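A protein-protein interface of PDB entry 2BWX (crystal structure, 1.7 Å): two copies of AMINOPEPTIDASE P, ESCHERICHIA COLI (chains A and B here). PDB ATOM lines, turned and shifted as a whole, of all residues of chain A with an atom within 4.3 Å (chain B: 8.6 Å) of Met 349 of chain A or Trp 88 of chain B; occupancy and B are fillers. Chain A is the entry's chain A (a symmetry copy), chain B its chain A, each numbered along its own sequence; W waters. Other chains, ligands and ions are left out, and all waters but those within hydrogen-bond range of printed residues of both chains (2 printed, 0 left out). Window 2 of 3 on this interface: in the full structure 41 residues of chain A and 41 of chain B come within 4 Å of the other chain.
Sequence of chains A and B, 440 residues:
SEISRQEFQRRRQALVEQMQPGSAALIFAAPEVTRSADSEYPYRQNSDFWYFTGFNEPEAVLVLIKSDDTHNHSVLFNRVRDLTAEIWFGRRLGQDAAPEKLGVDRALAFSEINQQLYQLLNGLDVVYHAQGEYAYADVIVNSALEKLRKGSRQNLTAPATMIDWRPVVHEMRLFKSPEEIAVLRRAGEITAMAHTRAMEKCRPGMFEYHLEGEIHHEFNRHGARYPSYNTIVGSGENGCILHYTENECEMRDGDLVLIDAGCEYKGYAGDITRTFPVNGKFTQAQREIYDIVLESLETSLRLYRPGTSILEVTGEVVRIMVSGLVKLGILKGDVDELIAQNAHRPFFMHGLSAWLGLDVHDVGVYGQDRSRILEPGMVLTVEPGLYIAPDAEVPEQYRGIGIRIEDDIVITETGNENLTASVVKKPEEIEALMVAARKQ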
ATOM      1  N   LEU A 242      15.544  23.306  26.264  1.00  0.00           N
ATOM      2  CA  LEU A 242      16.160  22.899  27.533  1.00  0.00           C
ATOM      3  C   LEU A 242      17.025  23.980  28.235  1.00  0.00           C
ATOM      4  O   LEU A 242      16.907  24.182  29.453  1.00  0.00           O
ATOM      5  CB  LEU A 242      16.967  21.603  27.349  1.00  0.00           C
ATOM      6  CG  LEU A 242      16.132  20.357  26.992  1.00  0.00           C
ATOM      7  CD1 LEU A 242      17.016  19.131  26.888  1.00  0.00           C
ATOM      8  CD2 LEU A 242      15.023  20.126  28.016  1.00  0.00           C
ATOM      9  N   HIS A 243      17.892  24.632  27.471  1.00  0.00           N
ATOM     10  CA  HIS A 243      18.742  25.725  27.996  1.00  0.00           C
ATOM     11  C   HIS A 243      18.328  27.074  27.383  1.00  0.00           C
ATOM     12  O   HIS A 243      19.169  27.846  26.915  1.00  0.00           O
ATOM     13  CB  HIS A 243      20.224  25.457  27.702  1.00  0.00           C
ATOM     14  CG  HIS A 243      20.764  24.214  28.342  1.00  0.00           C
ATOM     15  ND1 HIS A 243      20.623  22.960  27.779  1.00  0.00           N
ATOM     16  CD2 HIS A 243      21.474  24.036  29.483  1.00  0.00           C
ATOM     17  CE1 HIS A 243      21.203  22.064  28.557  1.00  0.00           C
ATOM     18  NE2 HIS A 243      21.730  22.691  29.595  1.00  0.00           N
ATOM     19  N   ARG A 345      11.513   8.871  24.993  1.00  0.00           N
ATOM     20  CA  ARG A 345      12.646   9.741  24.631  1.00  0.00           C
ATOM     21  C   ARG A 345      12.300  11.036  23.891  1.00  0.00           C
ATOM     22  O   ARG A 345      12.987  12.044  24.068  1.00  0.00           O
ATOM     23  CB  ARG A 345      13.688   8.978  23.809  1.00  0.00           C
ATOM     24  CG  ARG A 345      14.621   8.107  24.621  1.00  0.00           C
ATOM     25  CD  ARG A 345      15.855   7.741  23.803  1.00  0.00           C
ATOM     26  NE  ARG A 345      16.518   6.530  24.283  1.00  0.00           N
ATOM     27  CZ  ARG A 345      17.239   6.446  25.402  1.00  0.00           C
ATOM     28  NH1 ARG A 345      17.399   7.503  26.200  1.00  0.00           N
ATOM     29  NH2 ARG A 345      17.803   5.288  25.734  1.00  0.00           N
ATOM     30  N   PRO A 346      11.257  11.014  23.037  1.00  0.00           N
ATOM     31  CA  PRO A 346      10.835  12.277  22.411  1.00  0.00           C
ATOM     32  C   PRO A 346      10.352  13.337  23.405  1.00  0.00           C
ATOM     33  O   PRO A 346      10.387  14.529  23.086  1.00  0.00           O
ATOM     34  CB  PRO A 346       9.683  11.852  21.493  1.00  0.00           C
ATOM     35  CG  PRO A 346       9.914  10.393  21.256  1.00  0.00           C
ATOM     36  CD  PRO A 346      10.448   9.882  22.548  1.00  0.00           C
ATOM     37  N   PHE A 347       9.922  12.905  24.594  1.00  0.00           N
ATOM     38  CA  PHE A 347       9.360  13.802  25.606  1.00  0.00           C
ATOM     39  C   PHE A 347      10.253  13.988  26.825  1.00  0.00           C
ATOM     40  O   PHE A 347      10.167  15.020  27.477  1.00  0.00           O
ATOM     41  CB  PHE A 347       7.980  13.280  26.030  1.00  0.00           C
ATOM     42  CG  PHE A 347       7.087  12.977  24.864  1.00  0.00           C
ATOM     43  CD1 PHE A 347       6.629  14.013  24.049  1.00  0.00           C
ATOM     44  CD2 PHE A 347       6.741  11.674  24.547  1.00  0.00           C
ATOM     45  CE1 PHE A 347       5.815  13.747  22.949  1.00  0.00           C
ATOM     46  CE2 PHE A 347       5.932  11.399  23.454  1.00  0.00           C
ATOM     47  CZ  PHE A 347       5.469  12.436  22.651  1.00  0.00           C
ATOM     48  N   PHE A 348      11.084  12.989  27.141  1.00  0.00           N
ATOM     49  CA  PHE A 348      12.078  13.091  28.214  1.00  0.00           C
ATOM     50  C   PHE A 348      13.422  12.652  27.626  1.00  0.00           C
ATOM     51  O   PHE A 348      13.711  11.450  27.537  1.00  0.00           O
ATOM     52  CB  PHE A 348      11.684  12.210  29.404  1.00  0.00           C
ATOM     53  CG  PHE A 348      12.701  12.194  30.527  1.00  0.00           C
ATOM     54  CD1 PHE A 348      13.225  13.382  31.041  1.00  0.00           C
ATOM     55  CD2 PHE A 348      13.122  10.980  31.079  1.00  0.00           C
ATOM     56  CE1 PHE A 348      14.149  13.365  32.081  1.00  0.00           C
ATOM     57  CE2 PHE A 348      14.048  10.955  32.121  1.00  0.00           C
ATOM     58  CZ  PHE A 348      14.563  12.145  32.621  1.00  0.00           C
ATOM     59  N   MET A 349      14.215  13.631  27.190  1.00  0.00           N
ATOM     60  CA  MET A 349      15.385  13.350  26.350  1.00  0.00           C
ATOM     61  C   MET A 349      16.717  13.530  27.050  1.00  0.00           C
ATOM     62  O   MET A 349      17.777  13.372  26.419  1.00  0.00           O
ATOM     63  CB  MET A 349      15.350  14.208  25.068  1.00  0.00           C
ATOM     64  CG  MET A 349      15.508  15.717  25.260  1.00  0.00           C
ATOM     65  SD  MET A 349      14.062  16.495  25.993  1.00  0.00           S
ATOM     66  CE  MET A 349      12.781  16.104  24.806  1.00  0.00           C
ATOM     67  N   HIS A 350      16.686  13.860  28.338  1.00  0.00           N
ATOM     68  CA  HIS A 350      17.906  14.089  29.085  1.00  0.00           C
ATOM     69  C   HIS A 350      18.000  13.158  30.299  1.00  0.00           C
ATOM     70  O   HIS A 350      17.099  12.346  30.558  1.00  0.00           O
ATOM     71  CB  HIS A 350      18.051  15.571  29.475  1.00  0.00           C
ATOM     72  CG  HIS A 350      16.937  16.103  30.335  1.00  0.00           C
ATOM     73  ND1 HIS A 350      16.877  15.886  31.699  1.00  0.00           N
ATOM     74  CD2 HIS A 350      15.876  16.895  30.033  1.00  0.00           C
ATOM     75  CE1 HIS A 350      15.814  16.501  32.190  1.00  0.00           C
ATOM     76  NE2 HIS A 350      15.187  17.118  31.203  1.00  0.00           N
ATOM     77  N   TYR A 387       8.530  17.341  27.871  1.00  0.00           N
ATOM     78  CA  TYR A 387       8.516  18.467  26.926  1.00  0.00           C
ATOM     79  C   TYR A 387       7.754  18.016  25.700  1.00  0.00           C
ATOM     80  O   TYR A 387       8.197  17.121  24.989  1.00  0.00           O
ATOM     81  CB  TYR A 387       9.945  18.914  26.590  1.00  0.00           C
ATOM     82  CG  TYR A 387      10.833  18.950  27.812  1.00  0.00           C
ATOM     83  CD1 TYR A 387      11.584  17.821  28.182  1.00  0.00           C
ATOM     84  CD2 TYR A 387      10.883  20.072  28.642  1.00  0.00           C
ATOM     85  CE1 TYR A 387      12.379  17.819  29.308  1.00  0.00           C
ATOM     86  CE2 TYR A 387      11.684  20.081  29.786  1.00  0.00           C
ATOM     87  CZ  TYR A 387      12.416  18.938  30.123  1.00  0.00           C
ATOM     88  OH  TYR A 387      13.211  18.926  31.229  1.00  0.00           O
ATOM     89  N   ASP B  82      18.948  23.480  13.250  1.00  0.00           N
ATOM     90  CA  ASP B  82      19.167  22.103  13.660  1.00  0.00           C
ATOM     91  C   ASP B  82      18.219  21.810  14.812  1.00  0.00           C
ATOM     92  O   ASP B  82      18.379  22.353  15.907  1.00  0.00           O
ATOM     93  CB  ASP B  82      20.616  21.884  14.100  1.00  0.00           C
ATOM     94  CG  ASP B  82      20.891  20.437  14.494  1.00  0.00           C
ATOM     95  OD1 ASP B  82      20.792  20.106  15.700  1.00  0.00           O
ATOM     96  OD2 ASP B  82      21.171  19.623  13.587  1.00  0.00           O
ATOM     97  N   LEU B  83      17.242  20.950  14.560  1.00  0.00           N
ATOM     98  CA  LEU B  83      16.203  20.665  15.546  1.00  0.00           C
ATOM     99  C   LEU B  83      16.792  20.290  16.909  1.00  0.00           C
ATOM    100  O   LEU B  83      16.434  20.890  17.930  1.00  0.00           O
ATOM    101  CB  LEU B  83      15.280  19.554  15.050  1.00  0.00           C
ATOM    102  CG  LEU B  83      14.111  19.249  15.992  1.00  0.00           C
ATOM    103  CD1 LEU B  83      13.341  20.536  16.338  1.00  0.00           C
ATOM    104  CD2 LEU B  83      13.180  18.191  15.399  1.00  0.00           C
ATOM    105  N   THR B  84      17.709  19.323  16.917  1.00  0.00           N
ATOM    106  CA  THR B  84      18.279  18.833  18.173  1.00  0.00           C
ATOM    107  C   THR B  84      19.068  19.915  18.927  1.00  0.00           C
ATOM    108  O   THR B  84      18.828  20.146  20.113  1.00  0.00           O
ATOM    109  CB  THR B  84      19.156  17.576  17.946  1.00  0.00           C
ATOM    110  OG1 THR B  84      18.375  16.569  17.295  1.00  0.00           O
ATOM    111  CG2 THR B  84      19.671  17.020  19.272  1.00  0.00           C
ATOM    112  N   ALA B  85      19.993  20.582  18.242  1.00  0.00           N
ATOM    113  CA  ALA B  85      20.804  21.634  18.873  1.00  0.00           C
ATOM    114  C   ALA B  85      19.922  22.746  19.450  1.00  0.00           C
ATOM    115  O   ALA B  85      20.255  23.358  20.485  1.00  0.00           O
ATOM    116  CB  ALA B  85      21.807  22.225  17.870  1.00  0.00           C
ATOM    117  N   GLU B  86      18.798  22.992  18.773  1.00  0.00           N
ATOM    118  CA  GLU B  86      17.868  24.037  19.175  1.00  0.00           C
ATOM    119  C   GLU B  86      16.976  23.625  20.348  1.00  0.00           C
ATOM    120  O   GLU B  86      16.778  24.426  21.250  1.00  0.00           O
ATOM    121  CB  GLU B  86      17.047  24.532  17.978  1.00  0.00           C
ATOM    122  CG  GLU B  86      17.914  25.322  16.977  1.00  0.00           C
ATOM    123  CD  GLU B  86      17.107  25.873  15.841  1.00  0.00           C
ATOM    124  OE1 GLU B  86      16.165  26.649  16.116  1.00  0.00           O
ATOM    125  OE2 GLU B  86      17.409  25.515  14.677  1.00  0.00           O
ATOM    126  N   ILE B  87      16.454  22.398  20.342  1.00  0.00           N
ATOM    127  CA  ILE B  87      15.770  21.844  21.531  1.00  0.00           C
ATOM    128  C   ILE B  87      16.668  21.974  22.770  1.00  0.00           C
ATOM    129  O   ILE B  87      16.208  22.325  23.858  1.00  0.00           O
ATOM    130  CB  ILE B  87      15.375  20.360  21.340  1.00  0.00           C
ATOM    131  CG1 ILE B  87      14.220  20.248  20.343  1.00  0.00           C
ATOM    132  CG2 ILE B  87      14.991  19.703  22.678  1.00  0.00           C
ATOM    133  CD1 ILE B  87      14.096  18.873  19.709  1.00  0.00           C
ATOM    134  N   TRP B  88      17.951  21.699  22.598  1.00  0.00           N
ATOM    135  CA  TRP B  88      18.882  21.769  23.715  1.00  0.00           C
ATOM    136  C   TRP B  88      19.266  23.195  24.110  1.00  0.00           C
ATOM    137  O   TRP B  88      19.105  23.586  25.277  1.00  0.00           O
ATOM    138  CB  TRP B  88      20.111  20.891  23.424  1.00  0.00           C
ATOM    139  CG  TRP B  88      19.786  19.443  23.688  1.00  0.00           C
ATOM    140  CD1 TRP B  88      19.111  18.583  22.865  1.00  0.00           C
ATOM    141  CD2 TRP B  88      20.053  18.714  24.896  1.00  0.00           C
ATOM    142  NE1 TRP B  88      18.965  17.357  23.479  1.00  0.00           N
ATOM    143  CE2 TRP B  88      19.537  17.412  24.724  1.00  0.00           C
ATOM    144  CE3 TRP B  88      20.688  19.036  26.103  1.00  0.00           C
ATOM    145  CZ2 TRP B  88      19.637  16.425  25.716  1.00  0.00           C
ATOM    146  CZ3 TRP B  88      20.791  18.053  27.087  1.00  0.00           C
ATOM    147  CH2 TRP B  88      20.269  16.764  26.883  1.00  0.00           C
ATOM    148  N   PHE B  89      19.729  23.982  23.139  1.00  0.00           N
ATOM    149  CA  PHE B  89      20.496  25.203  23.443  1.00  0.00           C
ATOM    150  C   PHE B  89      19.886  26.516  22.975  1.00  0.00           C
ATOM    151  O   PHE B  89      20.397  27.599  23.308  1.00  0.00           O
ATOM    152  CB  PHE B  89      21.919  25.055  22.898  1.00  0.00           C
ATOM    153  CG  PHE B  89      22.635  23.843  23.441  1.00  0.00           C
ATOM    154  CD1 PHE B  89      22.849  23.706  24.818  1.00  0.00           C
ATOM    155  CD2 PHE B  89      23.067  22.829  22.596  1.00  0.00           C
ATOM    156  CE1 PHE B  89      23.493  22.589  25.337  1.00  0.00           C
ATOM    157  CE2 PHE B  89      23.714  21.711  23.108  1.00  0.00           C
ATOM    158  CZ  PHE B  89      23.927  21.593  24.482  1.00  0.00           C
ATOM    159  N   GLY B  90      18.794  26.431  22.224  1.00  0.00           N
ATOM    160  CA  GLY B  90      18.072  27.617  21.824  1.00  0.00           C
ATOM    161  C   GLY B  90      17.929  27.744  20.332  1.00  0.00           C
ATOM    162  O   GLY B  90      18.606  27.055  19.541  1.00  0.00           O
ATOM    163  N   ARG B  91      17.042  28.653  19.961  1.00  0.00           N
ATOM    164  CA  ARG B  91      16.680  28.834  18.584  1.00  0.00           C
ATOM    165  C   ARG B  91      17.829  29.500  17.842  1.00  0.00           C
ATOM    166  O   ARG B  91      18.630  30.251  18.420  1.00  0.00           O
ATOM    167  CB  ARG B  91      15.415  29.664  18.465  1.00  0.00           C
ATOM    168  CG  ARG B  91      14.211  29.024  19.122  1.00  0.00           C
ATOM    169  CD  ARG B  91      12.958  29.779  18.764  1.00  0.00           C
ATOM    170  NE  ARG B  91      11.795  29.234  19.444  1.00  0.00           N
ATOM    171  CZ  ARG B  91      11.425  29.534  20.691  1.00  0.00           C
ATOM    172  NH1 ARG B  91      12.130  30.397  21.424  1.00  0.00           N
ATOM    173  NH2 ARG B  91      10.335  28.970  21.197  1.00  0.00           N
HETATM  174  O   HOH W   1      19.312  29.982  24.808  1.00  0.00           O
HETATM  175  O   HOH W   2      21.982  27.324  25.982  1.00  0.00           O
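The backbone carbonyl oxygen of Ile 87 of chain B sits at hydrogen-bond distance from the backbone NH of Leu 242 of chain A (2.7 Å). O of Trp 88 of chain B sits at hydrogen-bond distance from N of His 243 of chain A (2.7 Å).
The side-chain hydroxyl (OH) of Tyr 387 of chain A is in hydrogen-bond range of a ring nitrogen (NE2) of His 350 of chain A, 2.7 Å away.
Trp 88 of chain B touches Leu 242 of chain A (O to CB, 3.6 Å). His 243 of chain A touches Phe 89 of chain B. Met 349 of chain A touches Trp 88 of chain B. CB of His 350 of chain A touches CH2 of Trp 88 of chain B (3.6 Å).
Of chain B, only Trp 88 comes within 4 Å of Met 349 of chain A. Trp 88 of chain B touches just these residues of chain A: Leu 242 (3.6 Å), His 243 (2.7 Å), Met 349 (3.6 Å) and His 350 (3.6 Å). Printed residues of chain B within 4 Å of His 350 of chain A: Trp 88. Of the printed residues of chain A, Ile 87 of chain B touches Leu 242 (2.7 Å). Arg 345 of chain A touches none of the printed residues of chain B. The nearest residue of chain B that does not touch Met 349 of chain A is Ile 87 of chain B (4.7 Å). The nearest printed residue of chain A that does not touch Trp 88 of chain B is Phe 348 of chain A (7.5 Å). The nearest printed residue of chain B that does not touch Leu 242 of chain A is Phe 89 of chain B (5.3 Å).
Of the 10 printed residues of chain B, 3 touch a printed residue of chain A. Printed residues of chain B that touch a printed residue of chain A: Ile 87, Trp 88 and Phe 89. Hydrophobic or aromatic side chains of chain B that line the printed part of chain A: Trp 88 and Phe 89. Hydrophobic or aromatic side chains of chain A within 4 Å of the printed part of chain B: Leu 242, His 243 and His 350. Among the printed residues, 6 pairs touch across the chains. Among the printed residues, no Asp or Glu carboxylate lies within 4 Å of a Lys or Arg side-chain nitrogen of the other chain.
No position is printed for both chains.
Water W1 bridges the backbone carbonyl oxygen (O) of His 243 of chain A and the backbone carbonyl oxygen (O) of Phe 89 of chain B. Water W2 lies within hydrogen-bond range of O of His 243 of chain A (3.0 Å) and O of Phe 89 of chain B (3.1 Å).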
